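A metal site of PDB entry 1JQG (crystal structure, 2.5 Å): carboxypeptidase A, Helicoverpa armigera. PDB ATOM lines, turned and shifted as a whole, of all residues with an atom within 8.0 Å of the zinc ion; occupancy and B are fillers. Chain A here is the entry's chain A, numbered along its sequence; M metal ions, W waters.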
ATOM      1  N   TRP A  52     -16.353  -9.058 -18.385  1.00  0.00           N
ATOM      2  CA  TRP A  52     -17.718  -9.374 -18.851  1.00  0.00           C
ATOM      3  C   TRP A  52     -17.860 -10.862 -19.192  1.00  0.00           C
ATOM      4  O   TRP A  52     -18.855 -11.460 -18.838  1.00  0.00           O
ATOM      5  CB  TRP A  52     -18.025  -8.543 -20.107  1.00  0.00           C
ATOM      6  CG  TRP A  52     -18.178  -7.083 -19.837  1.00  0.00           C
ATOM      7  CD1 TRP A  52     -18.020  -6.442 -18.633  1.00  0.00           C
ATOM      8  CD2 TRP A  52     -18.500  -6.050 -20.783  1.00  0.00           C
ATOM      9  NE1 TRP A  52     -18.227  -5.095 -18.774  1.00  0.00           N
ATOM     10  CE2 TRP A  52     -18.524  -4.831 -20.097  1.00  0.00           C
ATOM     11  CE3 TRP A  52     -18.779  -6.049 -22.148  1.00  0.00           C
ATOM     12  CZ2 TRP A  52     -18.835  -3.624 -20.718  1.00  0.00           C
ATOM     13  CZ3 TRP A  52     -19.068  -4.837 -22.785  1.00  0.00           C
ATOM     14  CH2 TRP A  52     -19.089  -3.628 -22.049  1.00  0.00           C
ATOM     15  N   LEU A 179     -31.907 -10.351 -11.488  1.00  0.00           N
ATOM     16  CA  LEU A 179     -31.299  -9.118 -11.040  1.00  0.00           C
ATOM     17  C   LEU A 179     -30.408  -9.253  -9.815  1.00  0.00           C
ATOM     18  O   LEU A 179     -30.139  -8.299  -9.126  1.00  0.00           O
ATOM     19  CB  LEU A 179     -32.348  -8.019 -10.857  1.00  0.00           C
ATOM     20  CG  LEU A 179     -32.925  -7.396 -12.142  1.00  0.00           C
ATOM     21  CD1 LEU A 179     -33.885  -6.258 -11.855  1.00  0.00           C
ATOM     22  CD2 LEU A 179     -31.871  -6.898 -13.128  1.00  0.00           C
ATOM     23  N   LEU A 180     -29.812 -10.401  -9.598  1.00  0.00           N
ATOM     24  CA  LEU A 180     -28.833 -10.634  -8.549  1.00  0.00           C
ATOM     25  C   LEU A 180     -27.606  -9.754  -8.844  1.00  0.00           C
ATOM     26  O   LEU A 180     -27.045  -9.132  -7.942  1.00  0.00           O
ATOM     27  CB  LEU A 180     -28.496 -12.121  -8.443  1.00  0.00           C
ATOM     28  CG  LEU A 180     -27.714 -12.559  -7.203  1.00  0.00           C
ATOM     29  CD1 LEU A 180     -28.514 -12.283  -5.972  1.00  0.00           C
ATOM     30  CD2 LEU A 180     -27.263 -14.016  -7.227  1.00  0.00           C
ATOM     31  N   HIS A 181     -27.193  -9.719 -10.102  1.00  0.00           N
ATOM     32  CA  HIS A 181     -26.205  -8.819 -10.639  1.00  0.00           C
ATOM     33  C   HIS A 181     -26.978  -7.687 -11.321  1.00  0.00           C
ATOM     34  O   HIS A 181     -27.482  -7.756 -12.463  1.00  0.00           O
ATOM     35  CB  HIS A 181     -25.296  -9.533 -11.609  1.00  0.00           C
ATOM     36  CG  HIS A 181     -24.282 -10.405 -10.965  1.00  0.00           C
ATOM     37  ND1 HIS A 181     -23.773 -11.536 -11.462  1.00  0.00           N
ATOM     38  CD2 HIS A 181     -23.596 -10.355  -9.801  1.00  0.00           C
ATOM     39  CE1 HIS A 181     -22.874 -12.210 -10.820  1.00  0.00           C
ATOM     40  NE2 HIS A 181     -22.760 -11.452  -9.739  1.00  0.00           N
ATOM     41  N   CYS A 182     -27.115  -6.563 -10.635  1.00  0.00           N
ATOM     42  CA  CYS A 182     -27.927  -5.443 -11.047  1.00  0.00           C
ATOM     43  C   CYS A 182     -27.748  -4.884 -12.422  1.00  0.00           C
ATOM     44  O   CYS A 182     -28.700  -4.293 -12.949  1.00  0.00           O
ATOM     45  CB  CYS A 182     -27.739  -4.437  -9.931  1.00  0.00           C
ATOM     46  SG  CYS A 182     -26.078  -3.970  -9.487  1.00  0.00           S
ATOM     47  N   ARG A 183     -26.635  -5.079 -13.086  1.00  0.00           N
ATOM     48  CA  ARG A 183     -26.395  -4.531 -14.426  1.00  0.00           C
ATOM     49  C   ARG A 183     -26.985  -5.407 -15.524  1.00  0.00           C
ATOM     50  O   ARG A 183     -27.068  -5.009 -16.691  1.00  0.00           O
ATOM     51  CB  ARG A 183     -24.933  -4.358 -14.763  1.00  0.00           C
ATOM     52  CG  ARG A 183     -24.072  -5.595 -14.766  1.00  0.00           C
ATOM     53  CD  ARG A 183     -22.600  -5.261 -14.908  1.00  0.00           C
ATOM     54  NE  ARG A 183     -21.783  -6.448 -15.187  1.00  0.00           N
ATOM     55  CZ  ARG A 183     -20.450  -6.400 -15.203  1.00  0.00           C
ATOM     56  NH1 ARG A 183     -19.809  -5.257 -15.008  1.00  0.00           N
ATOM     57  NH2 ARG A 183     -19.710  -7.445 -15.482  1.00  0.00           N
ATOM     58  N   GLU A 184     -27.397  -6.627 -15.153  1.00  0.00           N
ATOM     59  CA  GLU A 184     -28.022  -7.514 -16.129  1.00  0.00           C
ATOM     60  C   GLU A 184     -29.514  -7.263 -16.306  1.00  0.00           C
ATOM     61  O   GLU A 184     -30.343  -8.057 -15.838  1.00  0.00           O
ATOM     62  CB  GLU A 184     -27.763  -8.970 -15.738  1.00  0.00           C
ATOM     63  CG  GLU A 184     -26.315  -9.259 -15.534  1.00  0.00           C
ATOM     64  CD  GLU A 184     -26.085 -10.593 -14.877  1.00  0.00           C
ATOM     65  OE1 GLU A 184     -24.831 -10.761 -14.811  1.00  0.00           O
ATOM     66  OE2 GLU A 184     -27.057 -11.235 -14.514  1.00  0.00           O
ATOM     67  N   THR A 187     -32.599  -9.535 -17.549  1.00  0.00           N
ATOM     68  CA  THR A 187     -33.085 -10.635 -16.736  1.00  0.00           C
ATOM     69  C   THR A 187     -34.476 -10.371 -16.156  1.00  0.00           C
ATOM     70  O   THR A 187     -35.228 -11.364 -15.893  1.00  0.00           O
ATOM     71  CB  THR A 187     -32.126 -11.011 -15.601  1.00  0.00           C
ATOM     72  OG1 THR A 187     -31.973  -9.944 -14.673  1.00  0.00           O
ATOM     73  CG2 THR A 187     -30.793 -11.423 -16.204  1.00  0.00           C
ATOM     74  N   ARG A 235     -22.494  -4.178 -10.673  1.00  0.00           N
ATOM     75  CA  ARG A 235     -23.088  -5.515 -10.508  1.00  0.00           C
ATOM     76  C   ARG A 235     -23.257  -5.947  -9.061  1.00  0.00           C
ATOM     77  O   ARG A 235     -24.039  -6.848  -8.754  1.00  0.00           O
ATOM     78  CB  ARG A 235     -22.235  -6.549 -11.250  1.00  0.00           C
ATOM     79  CG  ARG A 235     -20.777  -6.607 -10.796  1.00  0.00           C
ATOM     80  CD  ARG A 235     -19.961  -7.580 -11.640  1.00  0.00           C
ATOM     81  NE  ARG A 235     -20.370  -8.950 -11.391  1.00  0.00           N
ATOM     82  CZ  ARG A 235     -19.500  -9.950 -11.242  1.00  0.00           C
ATOM     83  NH1 ARG A 235     -18.200  -9.668 -11.321  1.00  0.00           N
ATOM     84  NH2 ARG A 235     -19.895 -11.203 -11.019  1.00  0.00           N
ATOM     85  N   ASP A 252     -20.046  -9.030  -4.299  1.00  0.00           N
ATOM     86  CA  ASP A 252     -20.652  -9.820  -5.373  1.00  0.00           C
ATOM     87  C   ASP A 252     -21.563 -10.872  -4.725  1.00  0.00           C
ATOM     88  O   ASP A 252     -21.094 -11.847  -4.131  1.00  0.00           O
ATOM     89  CB  ASP A 252     -19.569 -10.504  -6.183  1.00  0.00           C
ATOM     90  CG  ASP A 252     -20.086 -11.229  -7.415  1.00  0.00           C
ATOM     91  OD1 ASP A 252     -19.230 -11.597  -8.233  1.00  0.00           O
ATOM     92  OD2 ASP A 252     -21.328 -11.393  -7.537  1.00  0.00           O
ATOM     93  N   ASN A 254     -23.289 -13.201  -5.925  1.00  0.00           N
ATOM     94  CA  ASN A 254     -23.191 -14.537  -6.507  1.00  0.00           C
ATOM     95  C   ASN A 254     -21.928 -15.227  -6.046  1.00  0.00           C
ATOM     96  O   ASN A 254     -21.484 -16.234  -6.606  1.00  0.00           O
ATOM     97  CB  ASN A 254     -23.317 -14.492  -8.030  1.00  0.00           C
ATOM     98  CG  ASN A 254     -23.984 -15.770  -8.562  1.00  0.00           C
ATOM     99  OD1 ASN A 254     -24.653 -16.489  -7.803  1.00  0.00           O
ATOM    100  ND2 ASN A 254     -23.833 -16.094  -9.840  1.00  0.00           N
ATOM    101  N   ASP A 304     -31.642 -19.327 -11.332  1.00  0.00           N
ATOM    102  CA  ASP A 304     -30.992 -18.027 -11.123  1.00  0.00           C
ATOM    103  C   ASP A 304     -30.713 -17.444 -12.497  1.00  0.00           C
ATOM    104  O   ASP A 304     -29.775 -17.866 -13.184  1.00  0.00           O
ATOM    105  CB  ASP A 304     -29.692 -18.221 -10.327  1.00  0.00           C
ATOM    106  CG  ASP A 304     -29.058 -16.919  -9.912  1.00  0.00           C
ATOM    107  OD1 ASP A 304     -29.669 -15.842 -10.005  1.00  0.00           O
ATOM    108  OD2 ASP A 304     -27.878 -16.959  -9.480  1.00  0.00           O
ATOM    109  N   ILE A 305     -31.538 -16.486 -12.894  1.00  0.00           N
ATOM    110  CA  ILE A 305     -31.463 -15.898 -14.224  1.00  0.00           C
ATOM    111  C   ILE A 305     -30.455 -14.774 -14.320  1.00  0.00           C
ATOM    112  O   ILE A 305     -30.648 -13.673 -13.811  1.00  0.00           O
ATOM    113  CB  ILE A 305     -32.865 -15.460 -14.738  1.00  0.00           C
ATOM    114  CG1 ILE A 305     -33.785 -16.716 -14.725  1.00  0.00           C
ATOM    115  CG2 ILE A 305     -32.823 -14.902 -16.148  1.00  0.00           C
ATOM    116  CD1 ILE A 305     -35.229 -16.456 -15.081  1.00  0.00           C
ATOM    117  N   HIS A 306     -29.414 -15.000 -15.123  1.00  0.00           N
ATOM    118  CA  HIS A 306     -28.410 -14.013 -15.413  1.00  0.00           C
ATOM    119  C   HIS A 306     -28.364 -13.705 -16.919  1.00  0.00           C
ATOM    120  O   HIS A 306     -29.061 -14.215 -17.751  1.00  0.00           O
ATOM    121  CB  HIS A 306     -26.993 -14.503 -15.016  1.00  0.00           C
ATOM    122  CG  HIS A 306     -26.840 -14.677 -13.538  1.00  0.00           C
ATOM    123  ND1 HIS A 306     -26.212 -13.792 -12.734  1.00  0.00           N
ATOM    124  CD2 HIS A 306     -27.234 -15.606 -12.634  1.00  0.00           C
ATOM    125  CE1 HIS A 306     -26.111 -14.075 -11.487  1.00  0.00           C
ATOM    126  NE2 HIS A 306     -26.776 -15.217 -11.399  1.00  0.00           N
ATOM    127  N   SER A 307     -27.516 -12.734 -17.201  1.00  0.00           N
ATOM    128  CA  SER A 307     -27.153 -12.258 -18.468  1.00  0.00           C
ATOM    129  C   SER A 307     -25.650 -11.814 -18.524  1.00  0.00           C
ATOM    130  O   SER A 307     -25.075 -11.574 -17.460  1.00  0.00           O
ATOM    131  CB  SER A 307     -27.899 -11.076 -19.083  1.00  0.00           C
ATOM    132  OG  SER A 307     -27.465  -9.820 -18.554  1.00  0.00           O
ATOM    133  N   PHE A 308     -24.675 -12.408 -19.191  1.00  0.00           N
ATOM    134  CA  PHE A 308     -24.861 -12.559 -20.624  1.00  0.00           C
ATOM    135  C   PHE A 308     -24.192 -13.799 -21.209  1.00  0.00           C
ATOM    136  O   PHE A 308     -23.114 -14.180 -20.647  1.00  0.00           O
ATOM    137  CB  PHE A 308     -24.820 -11.314 -21.517  1.00  0.00           C
ATOM    138  CG  PHE A 308     -23.431 -10.919 -21.865  1.00  0.00           C
ATOM    139  CD1 PHE A 308     -22.834 -11.489 -22.976  1.00  0.00           C
ATOM    140  CD2 PHE A 308     -22.677 -10.030 -21.118  1.00  0.00           C
ATOM    141  CE1 PHE A 308     -21.540 -11.186 -23.348  1.00  0.00           C
ATOM    142  CE2 PHE A 308     -21.385  -9.718 -21.479  1.00  0.00           C
ATOM    143  CZ  PHE A 308     -20.815 -10.282 -22.600  1.00  0.00           C
ATOM    144  N   THR A 380     -28.328 -21.997 -13.499  1.00  0.00           N
ATOM    145  CA  THR A 380     -28.034 -20.583 -13.625  1.00  0.00           C
ATOM    146  C   THR A 380     -28.158 -20.213 -15.112  1.00  0.00           C
ATOM    147  O   THR A 380     -27.380 -20.723 -15.916  1.00  0.00           O
ATOM    148  CB  THR A 380     -26.671 -20.243 -13.055  1.00  0.00           C
ATOM    149  OG1 THR A 380     -26.278 -18.996 -13.700  1.00  0.00           O
ATOM    150  CG2 THR A 380     -25.570 -21.254 -13.367  1.00  0.00           C
ATOM    151  N   TYR A 381     -29.199 -19.466 -15.475  1.00  0.00           N
ATOM    152  CA  TYR A 381     -29.450 -19.071 -16.837  1.00  0.00           C
ATOM    153  C   TYR A 381     -28.574 -17.899 -17.226  1.00  0.00           C
ATOM    154  O   TYR A 381     -28.307 -16.989 -16.464  1.00  0.00           O
ATOM    155  CB  TYR A 381     -30.910 -18.662 -17.064  1.00  0.00           C
ATOM    156  CG  TYR A 381     -31.837 -19.757 -17.537  1.00  0.00           C
ATOM    157  CD1 TYR A 381     -32.049 -20.901 -16.816  1.00  0.00           C
ATOM    158  CD2 TYR A 381     -32.521 -19.625 -18.713  1.00  0.00           C
ATOM    159  CE1 TYR A 381     -32.909 -21.910 -17.257  1.00  0.00           C
ATOM    160  CE2 TYR A 381     -33.390 -20.595 -19.182  1.00  0.00           C
ATOM    161  CZ  TYR A 381     -33.579 -21.732 -18.453  1.00  0.00           C
ATOM    162  OH  TYR A 381     -34.465 -22.714 -18.848  1.00  0.00           O
ATOM    163  N   GLU A 382     -28.096 -17.933 -18.459  1.00  0.00           N
ATOM    164  CA  GLU A 382     -27.319 -16.848 -19.041  1.00  0.00           C
ATOM    165  C   GLU A 382     -28.071 -16.457 -20.312  1.00  0.00           C
ATOM    166  O   GLU A 382     -27.842 -17.142 -21.292  1.00  0.00           O
ATOM    167  CB  GLU A 382     -25.889 -17.266 -19.352  1.00  0.00           C
ATOM    168  CG  GLU A 382     -25.054 -17.633 -18.116  1.00  0.00           C
ATOM    169  CD  GLU A 382     -24.684 -16.400 -17.296  1.00  0.00           C
ATOM    170  OE1 GLU A 382     -24.637 -15.322 -17.908  1.00  0.00           O
ATOM    171  OE2 GLU A 382     -24.445 -16.496 -16.064  1.00  0.00           O
ATOM    172  N   PHE A 395     -24.283  -5.725 -21.900  1.00  0.00           N
ATOM    173  CA  PHE A 395     -25.369  -5.687 -20.959  1.00  0.00           C
ATOM    174  C   PHE A 395     -26.452  -4.698 -21.358  1.00  0.00           C
ATOM    175  O   PHE A 395     -27.505  -4.694 -20.769  1.00  0.00           O
ATOM    176  CB  PHE A 395     -24.785  -5.340 -19.576  1.00  0.00           C
ATOM    177  CG  PHE A 395     -23.869  -6.409 -19.049  1.00  0.00           C
ATOM    178  CD1 PHE A 395     -24.345  -7.599 -18.511  1.00  0.00           C
ATOM    179  CD2 PHE A 395     -22.491  -6.160 -19.073  1.00  0.00           C
ATOM    180  CE1 PHE A 395     -23.461  -8.535 -18.047  1.00  0.00           C
ATOM    181  CE2 PHE A 395     -21.598  -7.131 -18.618  1.00  0.00           C
ATOM    182  CZ  PHE A 395     -22.086  -8.320 -18.109  1.00  0.00           C
HETATM  183 ZN    ZN M   1     -24.375 -12.463 -13.414  1.00  0.00          ZN
HETATM  184  O   HOH W   1     -22.571 -13.842 -14.313  1.00  0.00           O
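NE2 of His 181 sits at hydrogen-bond distance from NH2 of Arg 235 (3.1 Å).
The side-chain carboxylate of Asp 252 lies within hydrogen-bond range of a ring nitrogen (NE2) of His 181 (2.6 Å).
The side-chain carboxylate (OE2) of Glu 184 is in hydrogen-bond range of the backbone NH (N) of Ser 307, 3.1 Å away.
The backbone carbonyl oxygen of Glu 184 lies within hydrogen-bond range of the side-chain hydroxyl of Thr 187.
A ring nitrogen (NE2) of His 306 lies within hydrogen-bond range of the side-chain amide nitrogen (ND2) of Asn 254 (3.4 Å).
The backbone NH (N) of His 306 is in hydrogen-bond range of the backbone carbonyl oxygen (O) of Tyr 381 (2.6 Å).
A ring nitrogen (NE2) of His 306 lies within hydrogen-bond range of the side-chain carboxylate (OD2) of Asp 304.
Of the 20 residues printed, 3 come within 4 Å of the zinc ion.
Along chain A the residues within 4 Å of the zinc ion span positions 181 to 306.
The zinc ion is bound by ND1 of His 181, OE1 of Glu 184, ND1 of His 306 and water W1.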
